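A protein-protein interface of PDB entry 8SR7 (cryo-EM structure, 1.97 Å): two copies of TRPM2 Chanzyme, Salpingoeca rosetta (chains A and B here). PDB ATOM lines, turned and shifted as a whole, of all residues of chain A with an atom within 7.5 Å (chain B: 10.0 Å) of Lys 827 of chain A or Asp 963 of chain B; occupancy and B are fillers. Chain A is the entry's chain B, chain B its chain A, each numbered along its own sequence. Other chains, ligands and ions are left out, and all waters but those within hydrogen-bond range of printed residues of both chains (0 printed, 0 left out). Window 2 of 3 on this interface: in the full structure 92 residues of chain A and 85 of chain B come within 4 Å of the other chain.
N of Lys 827 of chain A lies within hydrogen-bond range of O of Glu 964 of chain B (3.1 Å).
OD1 of Asp 826 of chain A is in hydrogen-bond range of N of Phe 966 of chain B, at 2.8 Å.
The side-chain carboxylate of Asp 963 of chain B lies within salt-bridge range of the side-chain amino group of Lys 827 of chain A (3.4 Å).
The backbone carbonyl oxygen of Val 824 of chain A lies within hydrogen-bond range of the side-chain amino group of Lys 900 of chain A.
O of Phe 823 of chain A sits at hydrogen-bond distance from NZ of Lys 900 of chain A (3.3 Å).
O of Gln 957 of chain B sits at hydrogen-bond distance from OG of Ser 961 of chain B (3.0 Å).
The side-chain hydroxyl (OG) of Ser 961 of chain B is in hydrogen-bond range of the side-chain carboxylate (OE1) of Glu 964 of chain B (3.3 Å).
O of Leu 959 of chain B lies within hydrogen-bond range of NH2 of Arg 1008 of chain B (3.1 Å).
O of Leu 960 of chain B lies within hydrogen-bond range of NH2 of Arg 1008 of chain B (2.9 Å).
Among the printed residues, pairs that only touch across the chains: Tyr 822 of chain A with Phe 966 of chain B (3.8 Å), Val 824 of chain A with Ser 958 of chain B (3.5 Å), Leu 825 of chain A with Gln 957 of chain B (3.8 Å), Leu 825 of chain A with Ser 958 of chain B (3.8 Å), Leu 825 of chain A with Glu 964 of chain B (3.6 Å), Leu 825 of chain A with Phe 966 of chain B (3.6 Å), Leu 825 of chain A with Thr 970 of chain B (3.8 Å), Asp 826 of chain A with Glu 964 of chain B (3.8 Å), Asp 826 of chain A with Asp 965 of chain B (3.5 Å), Lys 827 of chain A with Asp 965 of chain B (3.4 Å), Gln 893 of chain A with Asp 963 of chain B (3.6 Å), Val 897 of chain A with Arg 1008 of chain B (3.9 Å), Val 897 of chain A with Thr 1010 of chain B (3.4 Å) and Lys 900 of chain A with Pro 962 of chain B (3.4 Å).
Lys 827 of chain A touches just these residues of chain B: Asp 963, Glu 964 and Asp 965.
Of chain A, only Lys 827 and Gln 893 come within 4 Å of Asp 963 of chain B.
Printed residues of chain A within 4 Å of Gln 957 of chain B: Leu 825 (3.8 Å).
Printed residues of chain B within 4 Å of Leu 825 of chain A: Gln 957 (3.8 Å), Ser 958 (3.8 Å), Glu 964 (3.6 Å), Phe 966 (3.6 Å) and Thr 970 (3.8 Å).
Of the printed residues of chain A, Phe 966 of chain B touches Tyr 822, Leu 825 and Asp 826.
Of the printed residues of chain B, Lys 900 of chain A touches Pro 962.
Printed residues of chain A within 4 Å of Glu 964 of chain B: Leu 825 (3.6 Å), Asp 826 (3.8 Å) and Lys 827 (3.1 Å).
Lys 896 of chain A touches none of the printed residues of chain B.
Hydrophobic or aromatic side chains of chain B that line the printed part of chain A: Pro 962 and Phe 966.
Hydrophobic or aromatic side chains of chain A within 4 Å of the printed part of chain B: Tyr 822, Val 824, Leu 825 and Val 897.
Among the printed residues, Asp or Glu carboxylates within 4 Å of a Lys or Arg side-chain nitrogen of the other chain: Lys 827 of chain A with Asp 963 of chain B (3.4 Å).
No position is printed for both chains.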
ATOM      1  N   TYR A 822      -4.889 -20.493 -20.978  1.00  0.00           N
ATOM      2  CA  TYR A 822      -3.788 -19.715 -20.396  1.00  0.00           C
ATOM      3  C   TYR A 822      -2.627 -20.620 -19.997  1.00  0.00           C
ATOM      4  O   TYR A 822      -1.466 -20.219 -20.138  1.00  0.00           O
ATOM      5  CB  TYR A 822      -4.279 -18.877 -19.202  1.00  0.00           C
ATOM      6  CG  TYR A 822      -3.195 -18.064 -18.480  1.00  0.00           C
ATOM      7  CD1 TYR A 822      -2.845 -16.787 -18.952  1.00  0.00           C
ATOM      8  CD2 TYR A 822      -2.618 -18.513 -17.256  1.00  0.00           C
ATOM      9  CE1 TYR A 822      -1.870 -16.014 -18.295  1.00  0.00           C
ATOM     10  CE2 TYR A 822      -1.639 -17.755 -16.601  1.00  0.00           C
ATOM     11  CZ  TYR A 822      -1.284 -16.509 -17.126  1.00  0.00           C
ATOM     12  OH  TYR A 822      -0.336 -15.752 -16.480  1.00  0.00           O
ATOM     13  N   PHE A 823      -2.947 -21.767 -19.375  1.00  0.00           N
ATOM     14  CA  PHE A 823      -1.971 -22.758 -18.912  1.00  0.00           C
ATOM     15  C   PHE A 823      -1.170 -23.349 -20.073  1.00  0.00           C
ATOM     16  O   PHE A 823       0.042 -23.565 -19.955  1.00  0.00           O
ATOM     17  CB  PHE A 823      -2.704 -23.855 -18.137  1.00  0.00           C
ATOM     18  CG  PHE A 823      -1.871 -25.064 -17.846  1.00  0.00           C
ATOM     19  CD1 PHE A 823      -0.814 -24.984 -16.927  1.00  0.00           C
ATOM     20  CD2 PHE A 823      -2.160 -26.293 -18.472  1.00  0.00           C
ATOM     21  CE1 PHE A 823      -0.035 -26.109 -16.642  1.00  0.00           C
ATOM     22  CE2 PHE A 823      -1.387 -27.427 -18.205  1.00  0.00           C
ATOM     23  CZ  PHE A 823      -0.324 -27.330 -17.291  1.00  0.00           C
ATOM     24  N   VAL A 824      -1.825 -23.640 -21.195  1.00  0.00           N
ATOM     25  CA  VAL A 824      -1.179 -24.240 -22.400  1.00  0.00           C
ATOM     26  C   VAL A 824      -0.436 -23.163 -23.192  1.00  0.00           C
ATOM     27  O   VAL A 824       0.538 -23.507 -23.823  1.00  0.00           O
ATOM     28  CB  VAL A 824      -2.192 -25.028 -23.250  1.00  0.00           C
ATOM     29  CG1 VAL A 824      -1.593 -25.603 -24.518  1.00  0.00           C
ATOM     30  CG2 VAL A 824      -2.846 -26.136 -22.451  1.00  0.00           C
ATOM     31  N   LEU A 825      -0.853 -21.904 -23.140  1.00  0.00           N
ATOM     32  CA  LEU A 825      -0.088 -20.828 -23.799  1.00  0.00           C
ATOM     33  C   LEU A 825       1.156 -20.397 -23.023  1.00  0.00           C
ATOM     34  O   LEU A 825       2.198 -20.132 -23.634  1.00  0.00           O
ATOM     35  CB  LEU A 825      -0.960 -19.607 -24.054  1.00  0.00           C
ATOM     36  CG  LEU A 825      -1.911 -19.768 -25.223  1.00  0.00           C
ATOM     37  CD1 LEU A 825      -2.884 -18.623 -25.266  1.00  0.00           C
ATOM     38  CD2 LEU A 825      -1.201 -19.968 -26.525  1.00  0.00           C
ATOM     39  N   ASP A 826       1.044 -20.239 -21.701  1.00  0.00           N
ATOM     40  CA  ASP A 826       2.187 -19.877 -20.869  1.00  0.00           C
ATOM     41  C   ASP A 826       3.107 -21.088 -20.742  1.00  0.00           C
ATOM     42  O   ASP A 826       2.653 -22.232 -20.856  1.00  0.00           O
ATOM     43  CB  ASP A 826       1.720 -19.389 -19.491  1.00  0.00           C
ATOM     44  CG  ASP A 826       2.814 -18.708 -18.692  1.00  0.00           C
ATOM     45  OD1 ASP A 826       3.368 -17.702 -19.181  1.00  0.00           O
ATOM     46  OD2 ASP A 826       3.114 -19.176 -17.576  1.00  0.00           O
ATOM     47  N   LYS A 827       4.411 -20.821 -20.612  1.00  0.00           N
ATOM     48  CA  LYS A 827       5.422 -21.870 -20.538  1.00  0.00           C
ATOM     49  C   LYS A 827       5.326 -22.657 -19.231  1.00  0.00           C
ATOM     50  O   LYS A 827       4.875 -22.155 -18.196  1.00  0.00           O
ATOM     51  CB  LYS A 827       6.829 -21.282 -20.729  1.00  0.00           C
ATOM     52  CG  LYS A 827       7.380 -20.418 -19.601  1.00  0.00           C
ATOM     53  CD  LYS A 827       8.779 -19.921 -19.914  1.00  0.00           C
ATOM     54  CE  LYS A 827       9.793 -21.045 -19.847  1.00  0.00           C
ATOM     55  NZ  LYS A 827      11.173 -20.551 -20.106  1.00  0.00           N
ATOM     56  N   LEU A 828       5.655 -23.934 -19.324  1.00  0.00           N
ATOM     57  CA  LEU A 828       5.671 -24.793 -18.158  1.00  0.00           C
ATOM     58  C   LEU A 828       6.930 -24.533 -17.348  1.00  0.00           C
ATOM     59  O   LEU A 828       7.997 -24.251 -17.899  1.00  0.00           O
ATOM     60  CB  LEU A 828       5.585 -26.256 -18.576  1.00  0.00           C
ATOM     61  CG  LEU A 828       4.252 -26.808 -19.067  1.00  0.00           C
ATOM     62  CD1 LEU A 828       4.466 -28.131 -19.767  1.00  0.00           C
ATOM     63  CD2 LEU A 828       3.335 -26.985 -17.894  1.00  0.00           C
ATOM     64  N   GLU A 829       6.799 -24.628 -16.035  1.00  0.00           N
ATOM     65  CA  GLU A 829       7.913 -24.442 -15.126  1.00  0.00           C
ATOM     66  C   GLU A 829       8.634 -25.765 -14.903  1.00  0.00           C
ATOM     67  O   GLU A 829       8.184 -26.830 -15.330  1.00  0.00           O
ATOM     68  CB  GLU A 829       7.428 -23.864 -13.797  1.00  0.00           C
ATOM     69  CG  GLU A 829       6.622 -22.586 -13.940  1.00  0.00           C
ATOM     70  CD  GLU A 829       5.938 -22.181 -12.649  1.00  0.00           C
ATOM     71  OE1 GLU A 829       5.928 -22.991 -11.699  1.00  0.00           O
ATOM     72  OE2 GLU A 829       5.409 -21.052 -12.585  1.00  0.00           O
ATOM     73  N   ASP A 830       9.785 -25.687 -14.220  1.00  0.00           N
ATOM     74  CA  ASP A 830      10.615 -26.850 -13.894  1.00  0.00           C
ATOM     75  C   ASP A 830      10.033 -27.769 -12.815  1.00  0.00           C
ATOM     76  O   ASP A 830      10.587 -28.850 -12.600  1.00  0.00           O
ATOM     77  CB  ASP A 830      12.006 -26.382 -13.471  1.00  0.00           C
ATOM     78  CG  ASP A 830      12.909 -26.099 -14.655  1.00  0.00           C
ATOM     79  OD1 ASP A 830      12.546 -26.474 -15.790  1.00  0.00           O
ATOM     80  OD2 ASP A 830      13.984 -25.496 -14.453  1.00  0.00           O
ATOM     81  N   SER A 833       3.343 -26.549 -11.325  1.00  0.00           N
ATOM     82  CA  SER A 833       2.896 -25.226 -10.913  1.00  0.00           C
ATOM     83  C   SER A 833       1.549 -25.315 -10.199  1.00  0.00           C
ATOM     84  O   SER A 833       0.905 -26.366 -10.180  1.00  0.00           O
ATOM     85  CB  SER A 833       2.798 -24.293 -12.118  1.00  0.00           C
ATOM     86  OG  SER A 833       1.972 -24.847 -13.126  1.00  0.00           O
ATOM     87  N   ILE A 835      -1.315 -23.625 -10.919  1.00  0.00           N
ATOM     88  CA  ILE A 835      -2.397 -23.708 -11.906  1.00  0.00           C
ATOM     89  C   ILE A 835      -2.590 -25.149 -12.400  1.00  0.00           C
ATOM     90  O   ILE A 835      -3.733 -25.584 -12.613  1.00  0.00           O
ATOM     91  CB  ILE A 835      -2.138 -22.661 -13.032  1.00  0.00           C
ATOM     92  CG1 ILE A 835      -3.241 -22.628 -14.104  1.00  0.00           C
ATOM     93  CG2 ILE A 835      -0.710 -22.739 -13.620  1.00  0.00           C
ATOM     94  CD1 ILE A 835      -3.087 -21.524 -15.118  1.00  0.00           C
ATOM     95  N   GLN A 893      12.966 -30.657 -20.886  1.00  0.00           N
ATOM     96  CA  GLN A 893      12.406 -29.751 -21.893  1.00  0.00           C
ATOM     97  C   GLN A 893      11.537 -30.493 -22.911  1.00  0.00           C
ATOM     98  O   GLN A 893      10.474 -29.986 -23.309  1.00  0.00           O
ATOM     99  CB  GLN A 893      13.555 -29.001 -22.578  1.00  0.00           C
ATOM    100  CG  GLN A 893      13.171 -28.012 -23.674  1.00  0.00           C
ATOM    101  CD  GLN A 893      12.401 -26.817 -23.146  1.00  0.00           C
ATOM    102  OE1 GLN A 893      12.654 -26.337 -22.042  1.00  0.00           O
ATOM    103  NE2 GLN A 893      11.451 -26.332 -23.936  1.00  0.00           N
ATOM    104  N   LYS A 896       8.065 -31.476 -21.537  1.00  0.00           N
ATOM    105  CA  LYS A 896       7.238 -30.264 -21.558  1.00  0.00           C
ATOM    106  C   LYS A 896       6.658 -30.010 -22.950  1.00  0.00           C
ATOM    107  O   LYS A 896       5.480 -29.638 -23.076  1.00  0.00           O
ATOM    108  CB  LYS A 896       8.090 -29.076 -21.109  1.00  0.00           C
ATOM    109  CG  LYS A 896       8.418 -29.046 -19.630  1.00  0.00           C
ATOM    110  CD  LYS A 896       8.986 -27.706 -19.208  1.00  0.00           C
ATOM    111  CE  LYS A 896      10.499 -27.718 -19.187  1.00  0.00           C
ATOM    112  NZ  LYS A 896      11.032 -26.564 -18.415  1.00  0.00           N
ATOM    113  N   VAL A 897       7.498 -30.189 -23.993  1.00  0.00           N
ATOM    114  CA  VAL A 897       7.106 -30.007 -25.400  1.00  0.00           C
ATOM    115  C   VAL A 897       6.054 -31.042 -25.840  1.00  0.00           C
ATOM    116  O   VAL A 897       5.038 -30.675 -26.464  1.00  0.00           O
ATOM    117  CB  VAL A 897       8.380 -30.008 -26.277  1.00  0.00           C
ATOM    118  CG1 VAL A 897       8.102 -30.120 -27.740  1.00  0.00           C
ATOM    119  CG2 VAL A 897       9.096 -28.685 -26.102  1.00  0.00           C
ATOM    120  N   LYS A 900       2.699 -30.309 -23.926  1.00  0.00           N
ATOM    121  CA  LYS A 900       1.978 -29.211 -24.578  1.00  0.00           C
ATOM    122  C   LYS A 900       1.369 -29.640 -25.914  1.00  0.00           C
ATOM    123  O   LYS A 900       0.328 -29.090 -26.310  1.00  0.00           O
ATOM    124  CB  LYS A 900       2.884 -27.998 -24.760  1.00  0.00           C
ATOM    125  CG  LYS A 900       2.979 -27.148 -23.513  1.00  0.00           C
ATOM    126  CD  LYS A 900       3.687 -25.840 -23.775  1.00  0.00           C
ATOM    127  CE  LYS A 900       3.740 -25.002 -22.514  1.00  0.00           C
ATOM    128  NZ  LYS A 900       2.395 -24.854 -21.904  1.00  0.00           N
ATOM    129  N   GLN B 957      -0.836 -21.594 -31.568  1.00  0.00           N
ATOM    130  CA  GLN B 957       0.102 -20.646 -30.958  1.00  0.00           C
ATOM    131  C   GLN B 957       0.977 -21.336 -29.913  1.00  0.00           C
ATOM    132  O   GLN B 957       2.167 -21.014 -29.779  1.00  0.00           O
ATOM    133  CB  GLN B 957      -0.676 -19.452 -30.379  1.00  0.00           C
ATOM    134  CG  GLN B 957       0.135 -18.344 -29.672  1.00  0.00           C
ATOM    135  CD  GLN B 957       1.078 -17.559 -30.572  1.00  0.00           C
ATOM    136  OE1 GLN B 957       0.875 -17.446 -31.781  1.00  0.00           O
ATOM    137  NE2 GLN B 957       2.131 -17.021 -29.974  1.00  0.00           N
ATOM    138  N   SER B 958       0.381 -22.268 -29.151  1.00  0.00           N
ATOM    139  CA  SER B 958       1.109 -23.077 -28.178  1.00  0.00           C
ATOM    140  C   SER B 958       2.090 -24.036 -28.844  1.00  0.00           C
ATOM    141  O   SER B 958       3.138 -24.333 -28.262  1.00  0.00           O
ATOM    142  CB  SER B 958       0.129 -23.851 -27.325  1.00  0.00           C
ATOM    143  OG  SER B 958      -0.436 -24.927 -28.048  1.00  0.00           O
ATOM    144  N   LEU B 959       1.694 -24.645 -29.977  1.00  0.00           N
ATOM    145  CA  LEU B 959       2.593 -25.551 -30.700  1.00  0.00           C
ATOM    146  C   LEU B 959       3.765 -24.800 -31.327  1.00  0.00           C
ATOM    147  O   LEU B 959       4.869 -25.350 -31.407  1.00  0.00           O
ATOM    148  CB  LEU B 959       1.859 -26.385 -31.746  1.00  0.00           C
ATOM    149  CG  LEU B 959       0.956 -27.527 -31.285  1.00  0.00           C
ATOM    150  CD1 LEU B 959       0.017 -27.951 -32.400  1.00  0.00           C
ATOM    151  CD2 LEU B 959       1.797 -28.683 -30.809  1.00  0.00           C
ATOM    152  N   LEU B 960       3.531 -23.568 -31.816  1.00  0.00           N
ATOM    153  CA  LEU B 960       4.597 -22.802 -32.469  1.00  0.00           C
ATOM    154  C   LEU B 960       5.600 -22.261 -31.453  1.00  0.00           C
ATOM    155  O   LEU B 960       6.809 -22.260 -31.710  1.00  0.00           O
ATOM    156  CB  LEU B 960       4.040 -21.654 -33.311  1.00  0.00           C
ATOM    157  CG  LEU B 960       3.318 -21.947 -34.624  1.00  0.00           C
ATOM    158  CD1 LEU B 960       2.482 -20.746 -35.004  1.00  0.00           C
ATOM    159  CD2 LEU B 960       4.299 -22.301 -35.722  1.00  0.00           C
ATOM    160  N   SER B 961       5.123 -21.795 -30.302  1.00  0.00           N
ATOM    161  CA  SER B 961       5.986 -21.234 -29.258  1.00  0.00           C
ATOM    162  C   SER B 961       5.689 -21.902 -27.915  1.00  0.00           C
ATOM    163  O   SER B 961       4.940 -21.350 -27.098  1.00  0.00           O
ATOM    164  CB  SER B 961       5.809 -19.720 -29.168  1.00  0.00           C
ATOM    165  OG  SER B 961       4.468 -19.383 -28.862  1.00  0.00           O
ATOM    166  N   PRO B 962       6.246 -23.091 -27.650  1.00  0.00           N
ATOM    167  CA  PRO B 962       5.928 -23.790 -26.396  1.00  0.00           C
ATOM    168  C   PRO B 962       6.756 -23.401 -25.181  1.00  0.00           C
ATOM    169  O   PRO B 962       6.548 -23.992 -24.118  1.00  0.00           O
ATOM    170  CB  PRO B 962       6.204 -25.255 -26.759  1.00  0.00           C
ATOM    171  CG  PRO B 962       7.303 -25.176 -27.711  1.00  0.00           C
ATOM    172  CD  PRO B 962       7.109 -23.934 -28.508  1.00  0.00           C
ATOM    173  N   ASP B 963       7.684 -22.456 -25.282  1.00  0.00           N
ATOM    174  CA  ASP B 963       8.542 -22.112 -24.152  1.00  0.00           C
ATOM    175  C   ASP B 963       8.637 -20.600 -23.997  1.00  0.00           C
ATOM    176  O   ASP B 963       9.716 -20.020 -23.861  1.00  0.00           O
ATOM    177  CB  ASP B 963       9.919 -22.751 -24.323  1.00  0.00           C
ATOM    178  CG  ASP B 963      10.633 -22.968 -23.000  1.00  0.00           C
ATOM    179  OD1 ASP B 963      10.052 -23.622 -22.108  1.00  0.00           O
ATOM    180  OD2 ASP B 963      11.774 -22.483 -22.852  1.00  0.00           O
ATOM    181  N   GLU B 964       7.489 -19.933 -24.038  1.00  0.00           N
ATOM    182  CA  GLU B 964       7.437 -18.483 -23.970  1.00  0.00           C
ATOM    183  C   GLU B 964       6.453 -18.074 -22.882  1.00  0.00           C
ATOM    184  O   GLU B 964       5.422 -18.729 -22.700  1.00  0.00           O
ATOM    185  CB  GLU B 964       7.026 -17.899 -25.349  1.00  0.00           C
ATOM    186  CG  GLU B 964       7.032 -16.373 -25.476  1.00  0.00           C
ATOM    187  CD  GLU B 964       6.492 -15.883 -26.802  1.00  0.00           C
ATOM    188  OE1 GLU B 964       6.039 -16.717 -27.610  1.00  0.00           O
ATOM    189  OE2 GLU B 964       6.521 -14.656 -27.038  1.00  0.00           O
ATOM    190  N   ASP B 965       6.823 -17.043 -22.114  1.00  0.00           N
ATOM    191  CA  ASP B 965       5.943 -16.420 -21.131  1.00  0.00           C
ATOM    192  C   ASP B 965       4.766 -15.741 -21.822  1.00  0.00           C
ATOM    193  O   ASP B 965       4.899 -15.266 -22.957  1.00  0.00           O
ATOM    194  CB  ASP B 965       6.707 -15.392 -20.297  1.00  0.00           C
ATOM    195  CG  ASP B 965       7.619 -16.029 -19.273  1.00  0.00           C
ATOM    196  OD1 ASP B 965       7.271 -17.111 -18.762  1.00  0.00           O
ATOM    197  OD2 ASP B 965       8.683 -15.446 -18.979  1.00  0.00           O
ATOM    198  N   PHE B 966       3.592 -15.843 -21.198  1.00  0.00           N
ATOM    199  CA  PHE B 966       2.358 -15.237 -21.743  1.00  0.00           C
ATOM    200  C   PHE B 966       2.447 -13.726 -21.664  1.00  0.00           C
ATOM    201  O   PHE B 966       2.846 -13.213 -20.624  1.00  0.00           O
ATOM    202  CB  PHE B 966       1.104 -15.778 -21.057  1.00  0.00           C
ATOM    203  CG  PHE B 966      -0.226 -15.403 -21.656  1.00  0.00           C
ATOM    204  CD1 PHE B 966      -0.773 -14.147 -21.460  1.00  0.00           C
ATOM    205  CD2 PHE B 966      -0.957 -16.327 -22.378  1.00  0.00           C
ATOM    206  CE1 PHE B 966      -1.999 -13.811 -22.009  1.00  0.00           C
ATOM    207  CE2 PHE B 966      -2.184 -15.991 -22.924  1.00  0.00           C
ATOM    208  CZ  PHE B 966      -2.702 -14.735 -22.739  1.00  0.00           C
ATOM    209  N   SER B 967       2.062 -13.052 -22.721  1.00  0.00           N
ATOM    210  CA  SER B 967       2.079 -11.613 -22.893  1.00  0.00           C
ATOM    211  C   SER B 967       0.918 -11.260 -23.807  1.00  0.00           C
ATOM    212  O   SER B 967       0.084 -12.114 -24.127  1.00  0.00           O
ATOM    213  CB  SER B 967       3.417 -11.137 -23.461  1.00  0.00           C
ATOM    214  OG  SER B 967       3.729 -11.821 -24.661  1.00  0.00           O
ATOM    215  N   ARG B 969       1.280 -10.246 -26.899  1.00  0.00           N
ATOM    216  CA  ARG B 969       1.661 -10.817 -28.197  1.00  0.00           C
ATOM    217  C   ARG B 969       1.149 -12.239 -28.401  1.00  0.00           C
ATOM    218  O   ARG B 969       0.899 -12.634 -29.548  1.00  0.00           O
ATOM    219  CB  ARG B 969       3.179 -10.792 -28.353  1.00  0.00           C
ATOM    220  CG  ARG B 969       3.804  -9.411 -28.205  1.00  0.00           C
ATOM    221  CD  ARG B 969       5.340  -9.367 -28.365  1.00  0.00           C
ATOM    222  NE  ARG B 969       6.059 -10.572 -27.954  1.00  0.00           N
ATOM    223  CZ  ARG B 969       6.689 -11.398 -28.781  1.00  0.00           C
ATOM    224  NH1 ARG B 969       6.709 -11.187 -30.087  1.00  0.00           N
ATOM    225  NH2 ARG B 969       7.311 -12.464 -28.285  1.00  0.00           N
ATOM    226  N   THR B 970       1.051 -13.015 -27.307  1.00  0.00           N
ATOM    227  CA  THR B 970       0.466 -14.358 -27.315  1.00  0.00           C
ATOM    228  C   THR B 970      -1.017 -14.307 -27.691  1.00  0.00           C
ATOM    229  O   THR B 970      -1.478 -15.109 -28.514  1.00  0.00           O
ATOM    230  CB  THR B 970       0.671 -14.999 -25.937  1.00  0.00           C
ATOM    231  OG1 THR B 970       2.063 -14.969 -25.607  1.00  0.00           O
ATOM    232  CG2 THR B 970       0.220 -16.448 -25.914  1.00  0.00           C
ATOM    233  N   ARG B1008      11.564 -29.379 -33.094  1.00  0.00           N
ATOM    234  CA  ARG B1008      10.596 -30.109 -32.286  1.00  0.00           C
ATOM    235  C   ARG B1008       9.641 -30.849 -33.206  1.00  0.00           C
ATOM    236  O   ARG B1008       9.297 -30.353 -34.278  1.00  0.00           O
ATOM    237  CB  ARG B1008       9.807 -29.178 -31.362  1.00  0.00           C
ATOM    238  CG  ARG B1008      10.662 -28.205 -30.577  1.00  0.00           C
ATOM    239  CD  ARG B1008       9.811 -27.223 -29.801  1.00  0.00           C
ATOM    240  NE  ARG B1008       8.782 -26.594 -30.619  1.00  0.00           N
ATOM    241  CZ  ARG B1008       8.944 -25.452 -31.272  1.00  0.00           C
ATOM    242  NH1 ARG B1008      10.083 -24.783 -31.218  1.00  0.00           N
ATOM    243  NH2 ARG B1008       7.931 -24.959 -31.980  1.00  0.00           N
ATOM    244  N   THR B1010       6.556 -31.782 -32.426  1.00  0.00           N
ATOM    245  CA  THR B1010       5.164 -31.385 -32.185  1.00  0.00           C
ATOM    246  C   THR B1010       4.670 -30.301 -33.130  1.00  0.00           C
ATOM    247  O   THR B1010       3.494 -30.341 -33.531  1.00  0.00           O
ATOM    248  CB  THR B1010       4.989 -30.868 -30.762  1.00  0.00           C
ATOM    249  OG1 THR B1010       6.078 -30.004 -30.455  1.00  0.00           O
ATOM    250  CG2 THR B1010       4.974 -32.017 -29.776  1.00  0.00           C
